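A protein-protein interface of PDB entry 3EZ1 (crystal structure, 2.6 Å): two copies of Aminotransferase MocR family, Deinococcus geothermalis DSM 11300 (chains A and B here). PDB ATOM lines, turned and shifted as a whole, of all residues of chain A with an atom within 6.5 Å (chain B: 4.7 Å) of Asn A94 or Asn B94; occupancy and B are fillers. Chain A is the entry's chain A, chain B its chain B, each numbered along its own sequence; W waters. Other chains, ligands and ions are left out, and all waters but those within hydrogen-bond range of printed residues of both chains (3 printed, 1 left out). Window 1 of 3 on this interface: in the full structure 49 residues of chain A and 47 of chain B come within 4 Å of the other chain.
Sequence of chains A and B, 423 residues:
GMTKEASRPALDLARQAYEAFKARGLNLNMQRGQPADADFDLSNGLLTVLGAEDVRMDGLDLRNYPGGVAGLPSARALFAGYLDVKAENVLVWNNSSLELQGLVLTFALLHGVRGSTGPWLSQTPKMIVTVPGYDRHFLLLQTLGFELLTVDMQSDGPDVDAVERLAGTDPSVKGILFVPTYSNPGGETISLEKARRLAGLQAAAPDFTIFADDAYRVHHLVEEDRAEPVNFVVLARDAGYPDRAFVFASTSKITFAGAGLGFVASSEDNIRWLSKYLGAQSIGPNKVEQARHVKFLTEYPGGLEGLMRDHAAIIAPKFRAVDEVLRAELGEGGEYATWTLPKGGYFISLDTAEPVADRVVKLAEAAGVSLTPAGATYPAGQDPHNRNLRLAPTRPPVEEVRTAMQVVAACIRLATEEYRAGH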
ATOM      1  N   VAL A  92      11.362 -27.620   6.722  1.00  0.00           N
ATOM      2  CA  VAL A  92      11.475 -26.156   6.712  1.00  0.00           C
ATOM      3  C   VAL A  92      12.171 -25.704   7.999  1.00  0.00           C
ATOM      4  O   VAL A  92      11.736 -26.073   9.097  1.00  0.00           O
ATOM      5  CB  VAL A  92      10.091 -25.472   6.599  1.00  0.00           C
ATOM      6  CG1 VAL A  92      10.252 -23.975   6.373  1.00  0.00           C
ATOM      7  CG2 VAL A  92       9.280 -26.079   5.461  1.00  0.00           C
ATOM      8  N   TRP A  93      13.228 -24.897   7.850  1.00  0.00           N
ATOM      9  CA  TRP A  93      14.031 -24.403   8.977  1.00  0.00           C
ATOM     10  C   TRP A  93      13.780 -22.882   9.187  1.00  0.00           C
ATOM     11  O   TRP A  93      12.608 -22.477   9.140  1.00  0.00           O
ATOM     12  CB  TRP A  93      15.496 -24.826   8.763  1.00  0.00           C
ATOM     13  CG  TRP A  93      16.321 -24.823  10.013  1.00  0.00           C
ATOM     14  CD1 TRP A  93      17.405 -24.038  10.273  1.00  0.00           C
ATOM     15  CD2 TRP A  93      16.104 -25.612  11.189  1.00  0.00           C
ATOM     16  NE1 TRP A  93      17.888 -24.293  11.528  1.00  0.00           N
ATOM     17  CE2 TRP A  93      17.112 -25.257  12.119  1.00  0.00           C
ATOM     18  CE3 TRP A  93      15.162 -26.594  11.546  1.00  0.00           C
ATOM     19  CZ2 TRP A  93      17.211 -25.850  13.390  1.00  0.00           C
ATOM     20  CZ3 TRP A  93      15.256 -27.186  12.813  1.00  0.00           C
ATOM     21  CH2 TRP A  93      16.275 -26.807  13.719  1.00  0.00           C
ATOM     22  N   ASN A  94      14.817 -22.052   9.404  1.00  0.00           N
ATOM     23  CA  ASN A  94      14.669 -20.614   9.690  1.00  0.00           C
ATOM     24  C   ASN A  94      14.923 -19.780   8.412  1.00  0.00           C
ATOM     25  O   ASN A  94      14.408 -20.156   7.364  1.00  0.00           O
ATOM     26  CB  ASN A  94      15.538 -20.203  10.907  1.00  0.00           C
ATOM     27  CG  ASN A  94      15.133 -20.908  12.194  1.00  0.00           C
ATOM     28  OD1 ASN A  94      13.953 -21.021  12.509  1.00  0.00           O
ATOM     29  ND2 ASN A  94      16.117 -21.346  12.962  1.00  0.00           N
ATOM     30  N   ASN A  95      15.753 -18.729   8.469  1.00  0.00           N
ATOM     31  CA  ASN A  95      15.918 -17.762   7.363  1.00  0.00           C
ATOM     32  C   ASN A  95      16.947 -18.033   6.255  1.00  0.00           C
ATOM     33  O   ASN A  95      17.064 -17.206   5.336  1.00  0.00           O
ATOM     34  CB  ASN A  95      16.231 -16.370   7.960  1.00  0.00           C
ATOM     35  CG  ASN A  95      17.657 -16.265   8.522  1.00  0.00           C
ATOM     36  OD1 ASN A  95      18.159 -17.199   9.151  1.00  0.00           O
ATOM     37  ND2 ASN A  95      18.303 -15.127   8.294  1.00  0.00           N
ATOM     38  N   SER A  96      17.671 -19.154   6.314  1.00  0.00           N
ATOM     39  CA  SER A  96      18.770 -19.408   5.367  1.00  0.00           C
ATOM     40  C   SER A  96      18.871 -20.839   4.801  1.00  0.00           C
ATOM     41  O   SER A  96      18.913 -21.816   5.552  1.00  0.00           O
ATOM     42  CB  SER A  96      20.084 -19.019   6.053  1.00  0.00           C
ATOM     43  OG  SER A  96      21.200 -19.191   5.198  1.00  0.00           O
ATOM     44  N   SER A  97      18.899 -20.931   3.470  1.00  0.00           N
ATOM     45  CA  SER A  97      19.125 -22.186   2.743  1.00  0.00           C
ATOM     46  C   SER A  97      20.600 -22.592   2.848  1.00  0.00           C
ATOM     47  O   SER A  97      20.898 -23.782   2.961  1.00  0.00           O
ATOM     48  CB  SER A  97      18.744 -22.038   1.268  1.00  0.00           C
ATOM     49  OG  SER A  97      18.945 -23.243   0.550  1.00  0.00           O
ATOM     50  N   GLU A  99      22.577 -21.970   5.342  1.00  0.00           N
ATOM     51  CA  GLU A  99      22.704 -22.507   6.716  1.00  0.00           C
ATOM     52  C   GLU A  99      22.278 -23.971   6.761  1.00  0.00           C
ATOM     53  O   GLU A  99      22.977 -24.793   7.354  1.00  0.00           O
ATOM     54  CB  GLU A  99      21.848 -21.703   7.702  1.00  0.00           C
ATOM     55  CG  GLU A  99      22.083 -22.024   9.169  1.00  0.00           C
ATOM     56  CD  GLU A  99      21.063 -21.376  10.083  1.00  0.00           C
ATOM     57  OE1 GLU A  99      19.862 -21.704   9.973  1.00  0.00           O
ATOM     58  OE2 GLU A  99      21.469 -20.567  10.935  1.00  0.00           O
ATOM     59  N   GLY A 258      17.142 -12.506   3.612  1.00  0.00           N
ATOM     60  CA  GLY A 258      17.623 -12.642   5.002  1.00  0.00           C
ATOM     61  C   GLY A 258      16.517 -12.772   6.049  1.00  0.00           C
ATOM     62  O   GLY A 258      16.810 -13.098   7.200  1.00  0.00           O
ATOM     63  N   GLY A 260      13.523 -14.469   5.015  1.00  0.00           N
ATOM     64  CA  GLY A 260      12.692 -15.451   4.319  1.00  0.00           C
ATOM     65  C   GLY A 260      12.695 -16.784   5.048  1.00  0.00           C
ATOM     66  O   GLY A 260      12.735 -16.809   6.277  1.00  0.00           O
ATOM     67  N   LEU A 261      12.667 -17.879   4.282  1.00  0.00           N
ATOM     68  CA  LEU A 261      12.652 -19.251   4.806  1.00  0.00           C
ATOM     69  C   LEU A 261      13.589 -20.151   4.008  1.00  0.00           C
ATOM     70  O   LEU A 261      13.578 -20.113   2.775  1.00  0.00           O
ATOM     71  CB  LEU A 261      11.247 -19.866   4.762  1.00  0.00           C
ATOM     72  CG  LEU A 261      10.140 -19.287   5.642  1.00  0.00           C
ATOM     73  CD1 LEU A 261       8.859 -20.056   5.385  1.00  0.00           C
ATOM     74  CD2 LEU A 261      10.494 -19.323   7.130  1.00  0.00           C
ATOM     75  N   GLY A 262      14.383 -20.950   4.725  1.00  0.00           N
ATOM     76  CA  GLY A 262      15.291 -21.942   4.147  1.00  0.00           C
ATOM     77  C   GLY A 262      14.697 -23.325   4.384  1.00  0.00           C
ATOM     78  O   GLY A 262      14.219 -23.616   5.495  1.00  0.00           O
ATOM     79  N   PHE A 263      14.724 -24.170   3.354  1.00  0.00           N
ATOM     80  CA  PHE A 263      14.160 -25.527   3.426  1.00  0.00           C
ATOM     81  C   PHE A 263      14.851 -26.510   2.480  1.00  0.00           C
ATOM     82  O   PHE A 263      15.567 -26.096   1.561  1.00  0.00           O
ATOM     83  CB  PHE A 263      12.643 -25.493   3.180  1.00  0.00           C
ATOM     84  CG  PHE A 263      12.244 -24.860   1.877  1.00  0.00           C
ATOM     85  CD1 PHE A 263      12.110 -23.468   1.771  1.00  0.00           C
ATOM     86  CD2 PHE A 263      11.978 -25.650   0.754  1.00  0.00           C
ATOM     87  CE1 PHE A 263      11.732 -22.871   0.556  1.00  0.00           C
ATOM     88  CE2 PHE A 263      11.600 -25.063  -0.465  1.00  0.00           C
ATOM     89  CZ  PHE A 263      11.477 -23.674  -0.564  1.00  0.00           C
ATOM     90  N   SER A 282      18.311 -28.301  18.909  1.00  0.00           N
ATOM     91  CA  SER A 282      17.189 -27.342  18.802  1.00  0.00           C
ATOM     92  C   SER A 282      15.831 -27.986  19.099  1.00  0.00           C
ATOM     93  O   SER A 282      15.597 -29.135  18.723  1.00  0.00           O
ATOM     94  CB  SER A 282      17.151 -26.720  17.396  1.00  0.00           C
ATOM     95  OG  SER A 282      16.110 -25.764  17.267  1.00  0.00           O
ATOM     96  N   GLY A 284      13.052 -26.752  17.875  1.00  0.00           N
ATOM     97  CA  GLY A 284      12.385 -26.619  16.579  1.00  0.00           C
ATOM     98  C   GLY A 284      12.684 -25.287  15.910  1.00  0.00           C
ATOM     99  O   GLY A 284      13.326 -24.425  16.520  1.00  0.00           O
ATOM    100  N   PRO A 285      12.218 -25.101  14.659  1.00  0.00           N
ATOM    101  CA  PRO A 285      12.448 -23.854  13.935  1.00  0.00           C
ATOM    102  C   PRO A 285      11.389 -22.804  14.283  1.00  0.00           C
ATOM    103  O   PRO A 285      10.432 -23.113  15.008  1.00  0.00           O
ATOM    104  CB  PRO A 285      12.339 -24.290  12.473  1.00  0.00           C
ATOM    105  CG  PRO A 285      11.362 -25.395  12.489  1.00  0.00           C
ATOM    106  CD  PRO A 285      11.421 -26.043  13.852  1.00  0.00           C
ATOM    107  N   ASN A 286      11.569 -21.579  13.776  1.00  0.00           N
ATOM    108  CA  ASN A 286      10.624 -20.484  14.022  1.00  0.00           C
ATOM    109  C   ASN A 286       9.321 -20.805  13.290  1.00  0.00           C
ATOM    110  O   ASN A 286       9.217 -20.700  12.071  1.00  0.00           O
ATOM    111  CB  ASN A 286      11.180 -19.112  13.629  1.00  0.00           C
ATOM    112  CG  ASN A 286      10.365 -17.955  14.209  1.00  0.00           C
ATOM    113  OD1 ASN A 286       9.135 -18.002  14.284  1.00  0.00           O
ATOM    114  ND2 ASN A 286      11.059 -16.904  14.619  1.00  0.00           N
ATOM    115  N   LYS A 287       8.335 -21.184  14.086  1.00  0.00           N
ATOM    116  CA  LYS A 287       7.040 -21.661  13.614  1.00  0.00           C
ATOM    117  C   LYS A 287       6.125 -20.484  13.222  1.00  0.00           C
ATOM    118  O   LYS A 287       5.246 -20.640  12.374  1.00  0.00           O
ATOM    119  CB  LYS A 287       6.449 -22.528  14.737  1.00  0.00           C
ATOM    120  CG  LYS A 287       5.545 -23.684  14.359  1.00  0.00           C
ATOM    121  CD  LYS A 287       5.621 -24.797  15.425  1.00  0.00           C
ATOM    122  CE  LYS A 287       5.260 -24.343  16.853  1.00  0.00           C
ATOM    123  NZ  LYS A 287       6.110 -25.045  17.841  1.00  0.00           N
ATOM    124  N   GLN A 290       7.230 -19.279   9.598  1.00  0.00           N
ATOM    125  CA  GLN A 290       6.717 -20.254   8.624  1.00  0.00           C
ATOM    126  C   GLN A 290       5.216 -20.052   8.388  1.00  0.00           C
ATOM    127  O   GLN A 290       4.759 -20.158   7.248  1.00  0.00           O
ATOM    128  CB  GLN A 290       7.008 -21.693   9.068  1.00  0.00           C
ATOM    129  CG  GLN A 290       8.492 -22.042   9.048  1.00  0.00           C
ATOM    130  CD  GLN A 290       8.811 -23.400   9.659  1.00  0.00           C
ATOM    131  OE1 GLN A 290       7.952 -24.280   9.756  1.00  0.00           O
ATOM    132  NE2 GLN A 290      10.064 -23.578  10.061  1.00  0.00           N
ATOM    133  N   TRP B  93      21.310 -14.275  17.158  1.00  0.00           N
ATOM    134  CA  TRP B  93      21.069 -15.208  16.044  1.00  0.00           C
ATOM    135  C   TRP B  93      19.544 -15.359  15.784  1.00  0.00           C
ATOM    136  O   TRP B  93      18.881 -14.329  15.690  1.00  0.00           O
ATOM    137  CB  TRP B  93      21.837 -16.514  16.311  1.00  0.00           C
ATOM    138  CG  TRP B  93      22.042 -17.360  15.094  1.00  0.00           C
ATOM    139  CD1 TRP B  93      21.511 -18.591  14.850  1.00  0.00           C
ATOM    140  CD2 TRP B  93      22.813 -17.019  13.940  1.00  0.00           C
ATOM    141  NE1 TRP B  93      21.909 -19.046  13.619  1.00  0.00           N
ATOM    142  CE2 TRP B  93      22.712 -18.104  13.033  1.00  0.00           C
ATOM    143  CE3 TRP B  93      23.588 -15.901  13.584  1.00  0.00           C
ATOM    144  CZ2 TRP B  93      23.365 -18.107  11.785  1.00  0.00           C
ATOM    145  CZ3 TRP B  93      24.233 -15.900  12.348  1.00  0.00           C
ATOM    146  CH2 TRP B  93      24.113 -16.997  11.461  1.00  0.00           C
ATOM    147  N   ASN B  94      18.988 -16.581  15.696  1.00  0.00           N
ATOM    148  CA  ASN B  94      17.568 -16.819  15.361  1.00  0.00           C
ATOM    149  C   ASN B  94      16.766 -17.307  16.591  1.00  0.00           C
ATOM    150  O   ASN B  94      17.044 -16.849  17.694  1.00  0.00           O
ATOM    151  CB  ASN B  94      17.458 -17.725  14.105  1.00  0.00           C
ATOM    152  CG  ASN B  94      17.953 -17.046  12.834  1.00  0.00           C
ATOM    153  OD1 ASN B  94      17.752 -15.847  12.628  1.00  0.00           O
ATOM    154  ND2 ASN B  94      18.560 -17.829  11.948  1.00  0.00           N
ATOM    155  N   ASN B  95      15.810 -18.227  16.427  1.00  0.00           N
ATOM    156  CA  ASN B  95      14.892 -18.619  17.505  1.00  0.00           C
ATOM    157  C   ASN B  95      15.401 -19.484  18.660  1.00  0.00           C
ATOM    158  O   ASN B  95      14.640 -19.693  19.606  1.00  0.00           O
ATOM    159  CB  ASN B  95      13.662 -19.334  16.908  1.00  0.00           C
ATOM    160  CG  ASN B  95      13.974 -20.752  16.430  1.00  0.00           C
ATOM    161  OD1 ASN B  95      14.998 -20.998  15.795  1.00  0.00           O
ATOM    162  ND2 ASN B  95      13.088 -21.684  16.737  1.00  0.00           N
ATOM    163  N   SER B  96      16.645 -19.967  18.613  1.00  0.00           N
ATOM    164  CA  SER B  96      17.132 -20.932  19.613  1.00  0.00           C
ATOM    165  C   SER B  96      18.508 -20.653  20.246  1.00  0.00           C
ATOM    166  O   SER B  96      19.510 -20.548  19.543  1.00  0.00           O
ATOM    167  CB  SER B  96      17.125 -22.317  18.952  1.00  0.00           C
ATOM    168  OG  SER B  96      17.638 -23.330  19.799  1.00  0.00           O
ATOM    169  N   GLU B  99      20.557 -23.900  19.893  1.00  0.00           N
ATOM    170  CA  GLU B  99      21.143 -23.944  18.528  1.00  0.00           C
ATOM    171  C   GLU B  99      22.469 -23.206  18.493  1.00  0.00           C
ATOM    172  O   GLU B  99      23.448 -23.735  17.961  1.00  0.00           O
ATOM    173  CB  GLU B  99      20.194 -23.320  17.494  1.00  0.00           C
ATOM    174  CG  GLU B  99      20.621 -23.461  16.033  1.00  0.00           C
ATOM    175  CD  GLU B  99      19.738 -22.667  15.090  1.00  0.00           C
ATOM    176  OE1 GLU B  99      19.669 -21.425  15.225  1.00  0.00           O
ATOM    177  OE2 GLU B  99      19.141 -23.281  14.186  1.00  0.00           O
ATOM    178  N   GLY B 260      11.270 -16.887  19.546  1.00  0.00           N
ATOM    179  CA  GLY B 260      11.948 -15.827  20.292  1.00  0.00           C
ATOM    180  C   GLY B 260      13.295 -15.510  19.660  1.00  0.00           C
ATOM    181  O   GLY B 260      13.421 -15.517  18.432  1.00  0.00           O
ATOM    182  N   LEU B 261      14.297 -15.251  20.501  1.00  0.00           N
ATOM    183  CA  LEU B 261      15.647 -14.893  20.063  1.00  0.00           C
ATOM    184  C   LEU B 261      16.709 -15.546  20.942  1.00  0.00           C
ATOM    185  O   LEU B 261      16.693 -15.374  22.161  1.00  0.00           O
ATOM    186  CB  LEU B 261      15.859 -13.372  20.088  1.00  0.00           C
ATOM    187  CG  LEU B 261      15.047 -12.468  19.158  1.00  0.00           C
ATOM    188  CD1 LEU B 261      15.454 -11.019  19.397  1.00  0.00           C
ATOM    189  CD2 LEU B 261      15.217 -12.837  17.678  1.00  0.00           C
ATOM    190  N   GLY B 262      17.601 -16.309  20.308  1.00  0.00           N
ATOM    191  CA  GLY B 262      18.759 -16.918  20.954  1.00  0.00           C
ATOM    192  C   GLY B 262      19.913 -15.953  20.738  1.00  0.00           C
ATOM    193  O   GLY B 262      20.011 -15.327  19.668  1.00  0.00           O
ATOM    194  N   PRO B 285      21.503 -13.427  10.352  1.00  0.00           N
ATOM    195  CA  PRO B 285      20.300 -13.879  11.053  1.00  0.00           C
ATOM    196  C   PRO B 285      19.037 -13.106  10.635  1.00  0.00           C
ATOM    197  O   PRO B 285      19.138 -12.103   9.911  1.00  0.00           O
ATOM    198  CB  PRO B 285      20.646 -13.609  12.521  1.00  0.00           C
ATOM    199  CG  PRO B 285      21.495 -12.408  12.474  1.00  0.00           C
ATOM    200  CD  PRO B 285      22.280 -12.489  11.184  1.00  0.00           C
ATOM    201  N   ASN B 286      17.871 -13.583  11.088  1.00  0.00           N
ATOM    202  CA  ASN B 286      16.581 -12.940  10.782  1.00  0.00           C
ATOM    203  C   ASN B 286      16.557 -11.559  11.452  1.00  0.00           C
ATOM    204  O   ASN B 286      16.303 -11.410  12.645  1.00  0.00           O
ATOM    205  CB  ASN B 286      15.376 -13.803  11.182  1.00  0.00           C
ATOM    206  CG  ASN B 286      14.070 -13.345  10.526  1.00  0.00           C
ATOM    207  OD1 ASN B 286      13.787 -12.151  10.394  1.00  0.00           O
ATOM    208  ND2 ASN B 286      13.263 -14.311  10.123  1.00  0.00           N
HETATM  209  O   HOH W   1      11.754 -14.983  16.415  1.00  0.00           O
HETATM  210  O   HOH W   2      18.760 -20.875  12.591  1.00  0.00           O
HETATM  211  O   HOH W   3      11.839 -15.932   8.523  1.00  0.00           O
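ND2 of Asn B94 touches CB of Asn A94, 3.98 Å away.
OE2 of Glu B99 touches ND2 of Asn A94 (3.8 Å).
Asn A95 touches Pro B285 (ND2 to C, 3.2 Å).
Gly A258 touches Pro B285.
Asn B286 touches Gly A258 (CA to O, 3.6 Å).
Ser A282 touches Ser B96.
OE2 of Glu B99 lies within hydrogen-bond range of NE1 of Trp A93.
The side-chain amide oxygen of Asn B95 lies within hydrogen-bond range of the side-chain amide nitrogen of Asn A94, at 3.1 Å.
The side-chain amide nitrogen of Asn B94 sits at hydrogen-bond distance from the side-chain amide oxygen of Asn A95, at 2.9 Å.
ND2 of Asn A95 sits close to N of Asn B286.
OE2 of Glu A99 sits at hydrogen-bond distance from NE1 of Trp B93 (3.1 Å).
O of Gly A284 lies within hydrogen-bond range of ND2 of Asn B95.
ND2 of Asn B95 sits close to O of Pro A285 (3.5 Å).
ND2 of Asn B95 sits close to N of Asn A286, 3.3 Å away.
Asn B94 touches its own counterpart, Asn A94.
Asn A94 touches Asn B95, and with the chains exchanged Asn A95 touches Asn B94.
Asn A94 touches Glu B99, but with the chains exchanged Glu A99 does not touch Asn B94 (4.1 Å).
Asn A95 touches Asn B286, and with the chains exchanged Asn A286 touches Asn B95.
Positions printed for both chains: 93, 94, 95, 96, 99, 260, 261, 262, 285 and 286.
Of the 14 pairs that touch across the chains among the printed residues, 9 have their exchanged pair printed and touching as well.
Water W3 lies within hydrogen-bond range of O of Gly A260 (2.6 Å) and ND2 of Asn B286 (2.7 Å).
Water W1 lies within hydrogen-bond range of O of Gly B260 (2.7 Å) and ND2 of Asn A286 (2.7 Å).
Water W2 lies within hydrogen-bond range of the side-chain amide nitrogen (ND2) of Asn A94 (2.7 Å), the side-chain carboxylate (OE1) of Glu B99 (2.8 Å), the side-chain carboxylate (OE1) of Glu A99 (3.0 Å) and the side-chain amide nitrogen (ND2) of Asn B94 (3.1 Å).
NE2 of Gln A290 is in hydrogen-bond range of O of Trp A93 (2.9 Å).
N of Asn A286 is in hydrogen-bond range of OD1 of Asn A94.
The side-chain hydroxyl (OG) of Ser A96 is in hydrogen-bond range of the backbone NH (N) of Glu A99 (3.1 Å).
The side-chain hydroxyl (OG) of Ser A282 lies within hydrogen-bond range of the backbone carbonyl oxygen (O) of Gly A284, at 3.2 Å.
The backbone NH of Trp B93 is in hydrogen-bond range of the backbone carbonyl oxygen of Gly B262 (3.0 Å).
The side-chain hydroxyl (OG) of Ser B96 is in hydrogen-bond range of the backbone NH (N) of Glu B99, at 3.0 Å.
Hydrophobic or aromatic side chains of chain B within 4 Å of the printed part of chain A: Trp B93.
Of the 18 printed residues of chain A, 9 touch a printed residue of chain B.
Among the printed residues, 14 pairs touch across the chains.
Among the printed residues, no Asp or Glu carboxylate lies within 4 Å of a Lys or Arg side-chain nitrogen of the other chain.
Printed residues of chain B within 4 Å of Asn A94: Asn B94 (3.98 Å), Asn B95 (3.1 Å) and Glu B99 (3.8 Å).
Of the printed residues of chain A, Asn B94 touches Asn A94 (3.98 Å) and Asn A95 (2.9 Å).
Of the printed residues of chain B, Asn A286 touches Asn B95.
Of the printed residues of chain B, Gly A284 touches Asn B95.
Of the printed residues of chain A, Pro B285 touches Asn A95 and Gly A258.
Printed residues of chain B within 4 Å of Asn A95: Asn B94 (2.9 Å), Pro B285 (3.2 Å) and Asn B286 (3.2 Å).
Gly A260 touches none of the printed residues of chain B.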
